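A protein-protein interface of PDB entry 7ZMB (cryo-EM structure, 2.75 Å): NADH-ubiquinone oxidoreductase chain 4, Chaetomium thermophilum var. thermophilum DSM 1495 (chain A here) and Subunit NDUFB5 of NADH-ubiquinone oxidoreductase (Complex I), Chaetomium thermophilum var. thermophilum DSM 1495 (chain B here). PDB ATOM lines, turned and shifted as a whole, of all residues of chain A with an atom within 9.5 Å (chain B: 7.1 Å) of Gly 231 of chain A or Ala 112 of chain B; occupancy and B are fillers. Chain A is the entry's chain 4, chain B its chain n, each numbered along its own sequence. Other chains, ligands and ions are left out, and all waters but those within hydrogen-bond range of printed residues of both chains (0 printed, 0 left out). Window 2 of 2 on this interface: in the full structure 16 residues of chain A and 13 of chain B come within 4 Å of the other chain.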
ATOM      1  N   LEU A 113      -4.215 -40.901   9.856  1.00  0.00           N
ATOM      2  CA  LEU A 113      -3.378 -39.717  10.012  1.00  0.00           C
ATOM      3  C   LEU A 113      -1.915 -39.963   9.671  1.00  0.00           C
ATOM      4  O   LEU A 113      -1.245 -40.778  10.308  1.00  0.00           O
ATOM      5  CB  LEU A 113      -3.492 -39.182  11.439  1.00  0.00           C
ATOM      6  CG  LEU A 113      -4.819 -38.501  11.764  1.00  0.00           C
ATOM      7  CD1 LEU A 113      -4.717 -37.703  13.045  1.00  0.00           C
ATOM      8  CD2 LEU A 113      -5.233 -37.614  10.607  1.00  0.00           C
ATOM      9  N   SER A 114      -1.419 -39.257   8.661  1.00  0.00           N
ATOM     10  CA  SER A 114      -0.004 -39.198   8.352  1.00  0.00           C
ATOM     11  C   SER A 114       0.532 -37.825   8.734  1.00  0.00           C
ATOM     12  O   SER A 114      -0.132 -37.032   9.403  1.00  0.00           O
ATOM     13  CB  SER A 114       0.240 -39.506   6.875  1.00  0.00           C
ATOM     14  OG  SER A 114      -0.110 -40.844   6.579  1.00  0.00           O
ATOM     15  N   PHE A 115       1.733 -37.505   8.271  1.00  0.00           N
ATOM     16  CA  PHE A 115       2.360 -36.231   8.690  1.00  0.00           C
ATOM     17  C   PHE A 115       1.811 -35.083   7.845  1.00  0.00           C
ATOM     18  O   PHE A 115       1.785 -33.941   8.335  1.00  0.00           O
ATOM     19  CB  PHE A 115       3.866 -36.308   8.428  1.00  0.00           C
ATOM     20  CG  PHE A 115       4.607 -37.371   9.200  1.00  0.00           C
ATOM     21  CD1 PHE A 115       4.543 -38.702   8.826  1.00  0.00           C
ATOM     22  CD2 PHE A 115       5.389 -37.034  10.292  1.00  0.00           C
ATOM     23  CE1 PHE A 115       5.224 -39.674   9.540  1.00  0.00           C
ATOM     24  CE2 PHE A 115       6.077 -38.004  11.001  1.00  0.00           C
ATOM     25  CZ  PHE A 115       5.994 -39.322  10.624  1.00  0.00           C
ATOM     26  N   TYR A 119      -7.007 -32.662   3.772  1.00  0.00           N
ATOM     27  CA  TYR A 119      -8.369 -32.527   4.256  1.00  0.00           C
ATOM     28  C   TYR A 119      -9.071 -31.458   3.437  1.00  0.00           C
ATOM     29  O   TYR A 119      -8.448 -30.479   3.025  1.00  0.00           O
ATOM     30  CB  TYR A 119      -8.385 -32.171   5.742  1.00  0.00           C
ATOM     31  CG  TYR A 119      -7.338 -32.921   6.534  1.00  0.00           C
ATOM     32  CD1 TYR A 119      -7.415 -34.295   6.687  1.00  0.00           C
ATOM     33  CD2 TYR A 119      -6.272 -32.260   7.120  1.00  0.00           C
ATOM     34  CE1 TYR A 119      -6.463 -34.986   7.403  1.00  0.00           C
ATOM     35  CE2 TYR A 119      -5.314 -32.944   7.841  1.00  0.00           C
ATOM     36  CZ  TYR A 119      -5.419 -34.307   7.983  1.00  0.00           C
ATOM     37  OH  TYR A 119      -4.475 -35.009   8.694  1.00  0.00           O
ATOM     38  N   ILE A 223       3.952 -19.599   8.692  1.00  0.00           N
ATOM     39  CA  ILE A 223       3.146 -20.802   8.847  1.00  0.00           C
ATOM     40  C   ILE A 223       3.895 -21.829   9.677  1.00  0.00           C
ATOM     41  O   ILE A 223       3.303 -22.554  10.484  1.00  0.00           O
ATOM     42  CB  ILE A 223       2.761 -21.344   7.460  1.00  0.00           C
ATOM     43  CG1 ILE A 223       1.937 -20.299   6.705  1.00  0.00           C
ATOM     44  CG2 ILE A 223       2.035 -22.670   7.568  1.00  0.00           C
ATOM     45  CD1 ILE A 223       1.832 -20.552   5.229  1.00  0.00           C
ATOM     46  N   LEU A 224       5.215 -21.895   9.501  1.00  0.00           N
ATOM     47  CA  LEU A 224       6.017 -22.853  10.244  1.00  0.00           C
ATOM     48  C   LEU A 224       6.124 -22.464  11.710  1.00  0.00           C
ATOM     49  O   LEU A 224       6.120 -23.330  12.588  1.00  0.00           O
ATOM     50  CB  LEU A 224       7.396 -22.982   9.602  1.00  0.00           C
ATOM     51  CG  LEU A 224       7.348 -23.645   8.229  1.00  0.00           C
ATOM     52  CD1 LEU A 224       8.732 -23.988   7.707  1.00  0.00           C
ATOM     53  CD2 LEU A 224       6.459 -24.864   8.275  1.00  0.00           C
ATOM     54  N   THR A 225       6.216 -21.167  11.996  1.00  0.00           N
ATOM     55  CA  THR A 225       6.178 -20.704  13.378  1.00  0.00           C
ATOM     56  C   THR A 225       4.854 -21.055  14.049  1.00  0.00           C
ATOM     57  O   THR A 225       4.837 -21.499  15.199  1.00  0.00           O
ATOM     58  CB  THR A 225       6.436 -19.200  13.424  1.00  0.00           C
ATOM     59  OG1 THR A 225       7.784 -18.945  13.025  1.00  0.00           O
ATOM     60  CG2 THR A 225       6.212 -18.646  14.815  1.00  0.00           C
ATOM     61  N   MET A 226       3.732 -20.880  13.347  1.00  0.00           N
ATOM     62  CA  MET A 226       2.442 -21.232  13.933  1.00  0.00           C
ATOM     63  C   MET A 226       2.379 -22.707  14.284  1.00  0.00           C
ATOM     64  O   MET A 226       1.864 -23.078  15.343  1.00  0.00           O
ATOM     65  CB  MET A 226       1.299 -20.903  12.976  1.00  0.00           C
ATOM     66  CG  MET A 226       1.205 -19.474  12.542  1.00  0.00           C
ATOM     67  SD  MET A 226      -0.310 -19.275  11.610  1.00  0.00           S
ATOM     68  CE  MET A 226      -0.113 -17.618  11.010  1.00  0.00           C
ATOM     69  N   SER A 227       2.866 -23.565  13.392  1.00  0.00           N
ATOM     70  CA  SER A 227       2.749 -24.993  13.620  1.00  0.00           C
ATOM     71  C   SER A 227       3.612 -25.444  14.787  1.00  0.00           C
ATOM     72  O   SER A 227       3.256 -26.396  15.483  1.00  0.00           O
ATOM     73  CB  SER A 227       3.106 -25.756  12.350  1.00  0.00           C
ATOM     74  OG  SER A 227       2.606 -27.077  12.406  1.00  0.00           O
ATOM     75  N   SER A 228       4.737 -24.776  15.022  1.00  0.00           N
ATOM     76  CA  SER A 228       5.576 -25.116  16.158  1.00  0.00           C
ATOM     77  C   SER A 228       4.987 -24.646  17.476  1.00  0.00           C
ATOM     78  O   SER A 228       5.331 -25.200  18.523  1.00  0.00           O
ATOM     79  CB  SER A 228       6.972 -24.531  15.979  1.00  0.00           C
ATOM     80  OG  SER A 228       6.889 -23.215  15.484  1.00  0.00           O
ATOM     81  N   ILE A 229       4.113 -23.646  17.454  1.00  0.00           N
ATOM     82  CA  ILE A 229       3.441 -23.203  18.669  1.00  0.00           C
ATOM     83  C   ILE A 229       2.198 -24.035  18.940  1.00  0.00           C
ATOM     84  O   ILE A 229       2.009 -24.554  20.040  1.00  0.00           O
ATOM     85  CB  ILE A 229       3.112 -21.697  18.576  1.00  0.00           C
ATOM     86  CG1 ILE A 229       4.378 -20.892  18.277  1.00  0.00           C
ATOM     87  CG2 ILE A 229       2.509 -21.207  19.870  1.00  0.00           C
ATOM     88  CD1 ILE A 229       4.150 -19.416  18.028  1.00  0.00           C
ATOM     89  N   VAL A 230       1.350 -24.198  17.928  1.00  0.00           N
ATOM     90  CA  VAL A 230       0.089 -24.909  18.089  1.00  0.00           C
ATOM     91  C   VAL A 230       0.281 -26.417  18.013  1.00  0.00           C
ATOM     92  O   VAL A 230      -0.495 -27.176  18.596  1.00  0.00           O
ATOM     93  CB  VAL A 230      -0.906 -24.401  17.032  1.00  0.00           C
ATOM     94  CG1 VAL A 230      -2.159 -25.255  16.980  1.00  0.00           C
ATOM     95  CG2 VAL A 230      -1.263 -22.971  17.313  1.00  0.00           C
ATOM     96  N   GLY A 231       1.306 -26.884  17.318  1.00  0.00           N
ATOM     97  CA  GLY A 231       1.483 -28.301  17.119  1.00  0.00           C
ATOM     98  C   GLY A 231       0.729 -28.868  15.944  1.00  0.00           C
ATOM     99  O   GLY A 231       0.818 -30.074  15.697  1.00  0.00           O
ATOM    100  N   THR A 232      -0.016 -28.041  15.225  1.00  0.00           N
ATOM    101  CA  THR A 232      -0.716 -28.451  14.021  1.00  0.00           C
ATOM    102  C   THR A 232      -1.051 -27.206  13.218  1.00  0.00           C
ATOM    103  O   THR A 232      -0.710 -26.082  13.597  1.00  0.00           O
ATOM    104  CB  THR A 232      -1.977 -29.262  14.342  1.00  0.00           C
ATOM    105  OG1 THR A 232      -2.680 -29.552  13.131  1.00  0.00           O
ATOM    106  CG2 THR A 232      -2.868 -28.513  15.272  1.00  0.00           C
ATOM    107  N   THR A 233      -1.709 -27.427  12.088  1.00  0.00           N
ATOM    108  CA  THR A 233      -2.199 -26.369  11.230  1.00  0.00           C
ATOM    109  C   THR A 233      -3.674 -26.506  10.897  1.00  0.00           C
ATOM    110  O   THR A 233      -4.232 -25.589  10.289  1.00  0.00           O
ATOM    111  CB  THR A 233      -1.393 -26.326   9.920  1.00  0.00           C
ATOM    112  OG1 THR A 233      -1.325 -27.644   9.353  1.00  0.00           O
ATOM    113  CG2 THR A 233       0.009 -25.769  10.144  1.00  0.00           C
ATOM    114  N   TYR A 234      -4.313 -27.614  11.273  1.00  0.00           N
ATOM    115  CA  TYR A 234      -5.723 -27.849  10.992  1.00  0.00           C
ATOM    116  C   TYR A 234      -6.557 -26.660  11.439  1.00  0.00           C
ATOM    117  O   TYR A 234      -6.391 -26.165  12.555  1.00  0.00           O
ATOM    118  CB  TYR A 234      -6.178 -29.126  11.703  1.00  0.00           C
ATOM    119  CG  TYR A 234      -7.543 -29.624  11.286  1.00  0.00           C
ATOM    120  CD1 TYR A 234      -7.766 -30.121  10.008  1.00  0.00           C
ATOM    121  CD2 TYR A 234      -8.605 -29.608  12.174  1.00  0.00           C
ATOM    122  CE1 TYR A 234      -9.001 -30.576   9.631  1.00  0.00           C
ATOM    123  CE2 TYR A 234      -9.844 -30.061  11.804  1.00  0.00           C
ATOM    124  CZ  TYR A 234     -10.040 -30.540  10.532  1.00  0.00           C
ATOM    125  OH  TYR A 234     -11.285 -30.991  10.169  1.00  0.00           O
ATOM    126  N   VAL A 237      -8.401 -26.711  14.912  1.00  0.00           N
ATOM    127  CA  VAL A 237      -7.484 -26.620  16.043  1.00  0.00           C
ATOM    128  C   VAL A 237      -6.792 -25.264  16.074  1.00  0.00           C
ATOM    129  O   VAL A 237      -6.671 -24.640  17.130  1.00  0.00           O
ATOM    130  CB  VAL A 237      -6.457 -27.762  15.988  1.00  0.00           C
ATOM    131  CG1 VAL A 237      -5.583 -27.741  17.223  1.00  0.00           C
ATOM    132  CG2 VAL A 237      -7.155 -29.093  15.813  1.00  0.00           C
ATOM    133  N   LEU A 238      -6.328 -24.787  14.922  1.00  0.00           N
ATOM    134  CA  LEU A 238      -5.451 -23.622  14.906  1.00  0.00           C
ATOM    135  C   LEU A 238      -6.201 -22.329  15.185  1.00  0.00           C
ATOM    136  O   LEU A 238      -5.644 -21.418  15.801  1.00  0.00           O
ATOM    137  CB  LEU A 238      -4.721 -23.547  13.566  1.00  0.00           C
ATOM    138  CG  LEU A 238      -3.851 -22.335  13.240  1.00  0.00           C
ATOM    139  CD1 LEU A 238      -2.520 -22.420  13.938  1.00  0.00           C
ATOM    140  CD2 LEU A 238      -3.665 -22.239  11.749  1.00  0.00           C
ATOM    141  N   LYS A 240      -8.715 -21.585  17.203  1.00  0.00           N
ATOM    142  CA  LYS A 240      -8.956 -21.374  18.625  1.00  0.00           C
ATOM    143  C   LYS A 240      -7.688 -21.145  19.438  1.00  0.00           C
ATOM    144  O   LYS A 240      -7.783 -20.878  20.639  1.00  0.00           O
ATOM    145  CB  LYS A 240      -9.751 -22.559  19.175  1.00  0.00           C
ATOM    146  CG  LYS A 240      -8.988 -23.854  19.177  1.00  0.00           C
ATOM    147  CD  LYS A 240      -9.834 -24.989  19.703  1.00  0.00           C
ATOM    148  CE  LYS A 240      -9.065 -26.288  19.647  1.00  0.00           C
ATOM    149  NZ  LYS A 240      -7.911 -26.302  20.575  1.00  0.00           N
ATOM    150  N   SER A 241      -6.514 -21.234  18.835  1.00  0.00           N
ATOM    151  CA  SER A 241      -5.299 -20.829  19.524  1.00  0.00           C
ATOM    152  C   SER A 241      -5.139 -19.319  19.460  1.00  0.00           C
ATOM    153  O   SER A 241      -5.376 -18.702  18.422  1.00  0.00           O
ATOM    154  CB  SER A 241      -4.076 -21.504  18.910  1.00  0.00           C
ATOM    155  OG  SER A 241      -3.948 -22.843  19.355  1.00  0.00           O
ATOM    156  N   PHE A 243      -2.352 -15.994  20.352  1.00  0.00           N
ATOM    157  CA  PHE A 243      -0.938 -15.751  20.149  1.00  0.00           C
ATOM    158  C   PHE A 243      -0.526 -14.510  20.917  1.00  0.00           C
ATOM    159  O   PHE A 243      -1.324 -13.593  21.120  1.00  0.00           O
ATOM    160  CB  PHE A 243      -0.605 -15.596  18.664  1.00  0.00           C
ATOM    161  CG  PHE A 243      -0.514 -16.895  17.934  1.00  0.00           C
ATOM    162  CD1 PHE A 243       0.410 -17.852  18.321  1.00  0.00           C
ATOM    163  CD2 PHE A 243      -1.356 -17.173  16.879  1.00  0.00           C
ATOM    164  CE1 PHE A 243       0.494 -19.052  17.663  1.00  0.00           C
ATOM    165  CE2 PHE A 243      -1.273 -18.376  16.220  1.00  0.00           C
ATOM    166  CZ  PHE A 243      -0.344 -19.314  16.612  1.00  0.00           C
ATOM    167  N   ALA B 106     -10.488 -33.872  17.168  1.00  0.00           N
ATOM    168  CA  ALA B 106      -9.929 -34.646  18.270  1.00  0.00           C
ATOM    169  C   ALA B 106      -8.738 -35.479  17.814  1.00  0.00           C
ATOM    170  O   ALA B 106      -7.708 -35.527  18.491  1.00  0.00           O
ATOM    171  CB  ALA B 106     -11.007 -35.540  18.873  1.00  0.00           C
ATOM    172  N   ALA B 107      -8.859 -36.131  16.661  1.00  0.00           N
ATOM    173  CA  ALA B 107      -7.787 -36.982  16.163  1.00  0.00           C
ATOM    174  C   ALA B 107      -6.511 -36.192  15.916  1.00  0.00           C
ATOM    175  O   ALA B 107      -5.412 -36.721  16.108  1.00  0.00           O
ATOM    176  CB  ALA B 107      -8.237 -37.687  14.883  1.00  0.00           C
ATOM    177  N   LEU B 108      -6.633 -34.935  15.493  1.00  0.00           N
ATOM    178  CA  LEU B 108      -5.471 -34.093  15.243  1.00  0.00           C
ATOM    179  C   LEU B 108      -5.005 -33.342  16.483  1.00  0.00           C
ATOM    180  O   LEU B 108      -3.818 -33.029  16.587  1.00  0.00           O
ATOM    181  CB  LEU B 108      -5.780 -33.107  14.118  1.00  0.00           C
ATOM    182  CG  LEU B 108      -6.173 -33.783  12.811  1.00  0.00           C
ATOM    183  CD1 LEU B 108      -7.044 -32.871  12.020  1.00  0.00           C
ATOM    184  CD2 LEU B 108      -4.959 -34.155  12.007  1.00  0.00           C
ATOM    185  N   GLU B 109      -5.907 -33.034  17.420  1.00  0.00           N
ATOM    186  CA  GLU B 109      -5.471 -32.638  18.753  1.00  0.00           C
ATOM    187  C   GLU B 109      -4.520 -33.679  19.328  1.00  0.00           C
ATOM    188  O   GLU B 109      -3.417 -33.358  19.784  1.00  0.00           O
ATOM    189  CB  GLU B 109      -6.664 -32.484  19.695  1.00  0.00           C
ATOM    190  CG  GLU B 109      -7.663 -31.376  19.435  1.00  0.00           C
ATOM    191  CD  GLU B 109      -7.092 -29.992  19.631  1.00  0.00           C
ATOM    192  OE1 GLU B 109      -6.194 -29.823  20.481  1.00  0.00           O
ATOM    193  OE2 GLU B 109      -7.600 -29.060  18.985  1.00  0.00           O
ATOM    194  N   GLN B 110      -4.942 -34.944  19.310  1.00  0.00           N
ATOM    195  CA  GLN B 110      -4.133 -35.997  19.906  1.00  0.00           C
ATOM    196  C   GLN B 110      -2.816 -36.160  19.164  1.00  0.00           C
ATOM    197  O   GLN B 110      -1.758 -36.298  19.789  1.00  0.00           O
ATOM    198  CB  GLN B 110      -4.910 -37.311  19.930  1.00  0.00           C
ATOM    199  CG  GLN B 110      -4.321 -38.339  20.872  1.00  0.00           C
ATOM    200  CD  GLN B 110      -4.019 -37.762  22.242  1.00  0.00           C
ATOM    201  OE1 GLN B 110      -2.890 -37.361  22.525  1.00  0.00           O
ATOM    202  NE2 GLN B 110      -5.031 -37.718  23.102  1.00  0.00           N
ATOM    203  N   ALA B 111      -2.856 -36.114  17.833  1.00  0.00           N
ATOM    204  CA  ALA B 111      -1.626 -36.184  17.056  1.00  0.00           C
ATOM    205  C   ALA B 111      -0.706 -35.017  17.377  1.00  0.00           C
ATOM    206  O   ALA B 111       0.509 -35.192  17.496  1.00  0.00           O
ATOM    207  CB  ALA B 111      -1.946 -36.222  15.564  1.00  0.00           C
ATOM    208  N   ALA B 112      -1.271 -33.818  17.530  1.00  0.00           N
ATOM    209  CA  ALA B 112      -0.457 -32.651  17.852  1.00  0.00           C
ATOM    210  C   ALA B 112       0.229 -32.813  19.201  1.00  0.00           C
ATOM    211  O   ALA B 112       1.369 -32.375  19.382  1.00  0.00           O
ATOM    212  CB  ALA B 112      -1.315 -31.389  17.837  1.00  0.00           C
ATOM    213  N   HIS B 113      -0.456 -33.446  20.151  1.00  0.00           N
ATOM    214  CA  HIS B 113       0.135 -33.689  21.492  1.00  0.00           C
ATOM    215  C   HIS B 113       1.258 -34.721  21.381  1.00  0.00           C
ATOM    216  O   HIS B 113       2.277 -34.554  22.061  1.00  0.00           O
ATOM    217  CB  HIS B 113      -0.944 -34.142  22.481  1.00  0.00           C
ATOM    218  CG  HIS B 113      -0.389 -34.717  23.740  1.00  0.00           C
ATOM    219  ND1 HIS B 113       0.214 -33.935  24.705  1.00  0.00           N
ATOM    220  CD2 HIS B 113      -0.332 -35.989  24.189  1.00  0.00           C
ATOM    221  CE1 HIS B 113       0.615 -34.701  25.698  1.00  0.00           C
ATOM    222  NE2 HIS B 113       0.292 -35.965  25.406  1.00  0.00           N
ATOM    223  N   ASP B 114       1.055 -35.757  20.567  1.00  0.00           N
ATOM    224  CA  ASP B 114       2.086 -36.779  20.414  1.00  0.00           C
ATOM    225  C   ASP B 114       3.354 -36.186  19.826  1.00  0.00           C
ATOM    226  O   ASP B 114       4.459 -36.450  20.309  1.00  0.00           O
ATOM    227  CB  ASP B 114       1.572 -37.922  19.541  1.00  0.00           C
ATOM    228  CG  ASP B 114       0.247 -38.474  20.022  1.00  0.00           C
ATOM    229  OD1 ASP B 114      -0.020 -38.408  21.240  1.00  0.00           O
ATOM    230  OD2 ASP B 114      -0.531 -38.971  19.181  1.00  0.00           O
ATOM    231  N   LYS B 115       3.209 -35.366  18.784  1.00  0.00           N
ATOM    232  CA  LYS B 115       4.364 -34.697  18.202  1.00  0.00           C
ATOM    233  C   LYS B 115       5.018 -33.779  19.217  1.00  0.00           C
ATOM    234  O   LYS B 115       6.248 -33.719  19.310  1.00  0.00           O
ATOM    235  CB  LYS B 115       3.940 -33.925  16.953  1.00  0.00           C
ATOM    236  CG  LYS B 115       4.989 -32.974  16.394  1.00  0.00           C
ATOM    237  CD  LYS B 115       4.497 -32.309  15.116  1.00  0.00           C
ATOM    238  CE  LYS B 115       5.230 -31.004  14.839  1.00  0.00           C
ATOM    239  NZ  LYS B 115       4.583 -29.833  15.503  1.00  0.00           N
ATOM    240  N   HIS B 116       4.209 -33.075  20.009  1.00  0.00           N
ATOM    241  CA  HIS B 116       4.745 -32.208  21.053  1.00  0.00           C
ATOM    242  C   HIS B 116       5.556 -33.006  22.068  1.00  0.00           C
ATOM    243  O   HIS B 116       6.620 -32.564  22.507  1.00  0.00           O
ATOM    244  CB  HIS B 116       3.592 -31.454  21.712  1.00  0.00           C
ATOM    245  CG  HIS B 116       3.932 -30.826  23.025  1.00  0.00           C
ATOM    246  ND1 HIS B 116       3.112 -30.930  24.128  1.00  0.00           N
ATOM    247  CD2 HIS B 116       4.986 -30.071  23.410  1.00  0.00           C
ATOM    248  CE1 HIS B 116       3.649 -30.272  25.135  1.00  0.00           C
ATOM    249  NE2 HIS B 116       4.788 -29.744  24.728  1.00  0.00           N
ATOM    250  N   LEU B 117       5.076 -34.195  22.429  1.00  0.00           N
ATOM    251  CA  LEU B 117       5.835 -35.094  23.292  1.00  0.00           C
ATOM    252  C   LEU B 117       7.159 -35.515  22.661  1.00  0.00           C
ATOM    253  O   LEU B 117       8.197 -35.529  23.331  1.00  0.00           O
ATOM    254  CB  LEU B 117       4.989 -36.327  23.599  1.00  0.00           C
ATOM    255  CG  LEU B 117       5.082 -37.064  24.932  1.00  0.00           C
ATOM    256  CD1 LEU B 117       4.823 -36.158  26.089  1.00  0.00           C
ATOM    257  CD2 LEU B 117       4.093 -38.211  24.929  1.00  0.00           C
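Of the printed residues of chain B, Leu 113 of chain A touches Ala 107 (3.3 Å) and Leu 108 (3.7 Å).
Thr 232 of chain A touches none of the printed residues of chain B.
Of the printed residues of chain B, Tyr 234 of chain A touches Leu 108.
Of the printed residues of chain B, Lys 240 of chain A touches Glu 109.
Of the printed residues of chain A, Ala 107 of chain B touches Leu 113.
Gln 110 of chain B touches none of the printed residues of chain A.
No residue of chain A comes within 4 Å of Ala 111 of chain B.
Ala 112 of chain B touches just one residue of chain A: Gly 231 (3.3 Å).
Of chain A, only Ser 227 and Gly 231 come within 4 Å of Lys 115 of chain B.
The nearest residue of chain B that does not touch Gly 231 of chain A is Ala 111 of chain B (5.4 Å).
The nearest printed residue of chain B that does not touch Leu 113 of chain A is Ala 111 of chain B (4.03 Å).
Among the printed residues, pairs that only touch across the chains: Val 237 of chain A with Glu 109 of chain B, Leu 113 of chain A with Ala 107 of chain B, Gly 231 of chain A with Ala 112 of chain B, Tyr 234 of chain A with Leu 108 of chain B, Tyr 119 of chain A with Leu 108 of chain B, Ser 227 of chain A with Lys 115 of chain B, Leu 113 of chain A with Leu 108 of chain B and Gly 231 of chain A with Lys 115 of chain B.
NZ of Lys 240 of chain A is in salt-bridge range of OE2 of Glu 109 of chain B.
The backbone NH (N) of Tyr 234 of chain A lies within hydrogen-bond range of the side-chain hydroxyl (OG1) of Thr 232 of chain A (3.1 Å).
Hydrophobic or aromatic side chains of chain B that line the printed part of chain A: Ala 107, Leu 108 and Ala 112.
Along chain B the printed residues that touch a printed residue of chain A span positions 107 to 115.
Of the 21 printed residues of chain A, 7 touch a printed residue of chain B.
Hydrophobic or aromatic side chains of chain A that line the printed part of chain B: Leu 113, Tyr 119, Tyr 234 and Val 237.
Among the printed residues, 9 pairs touch across the chains.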
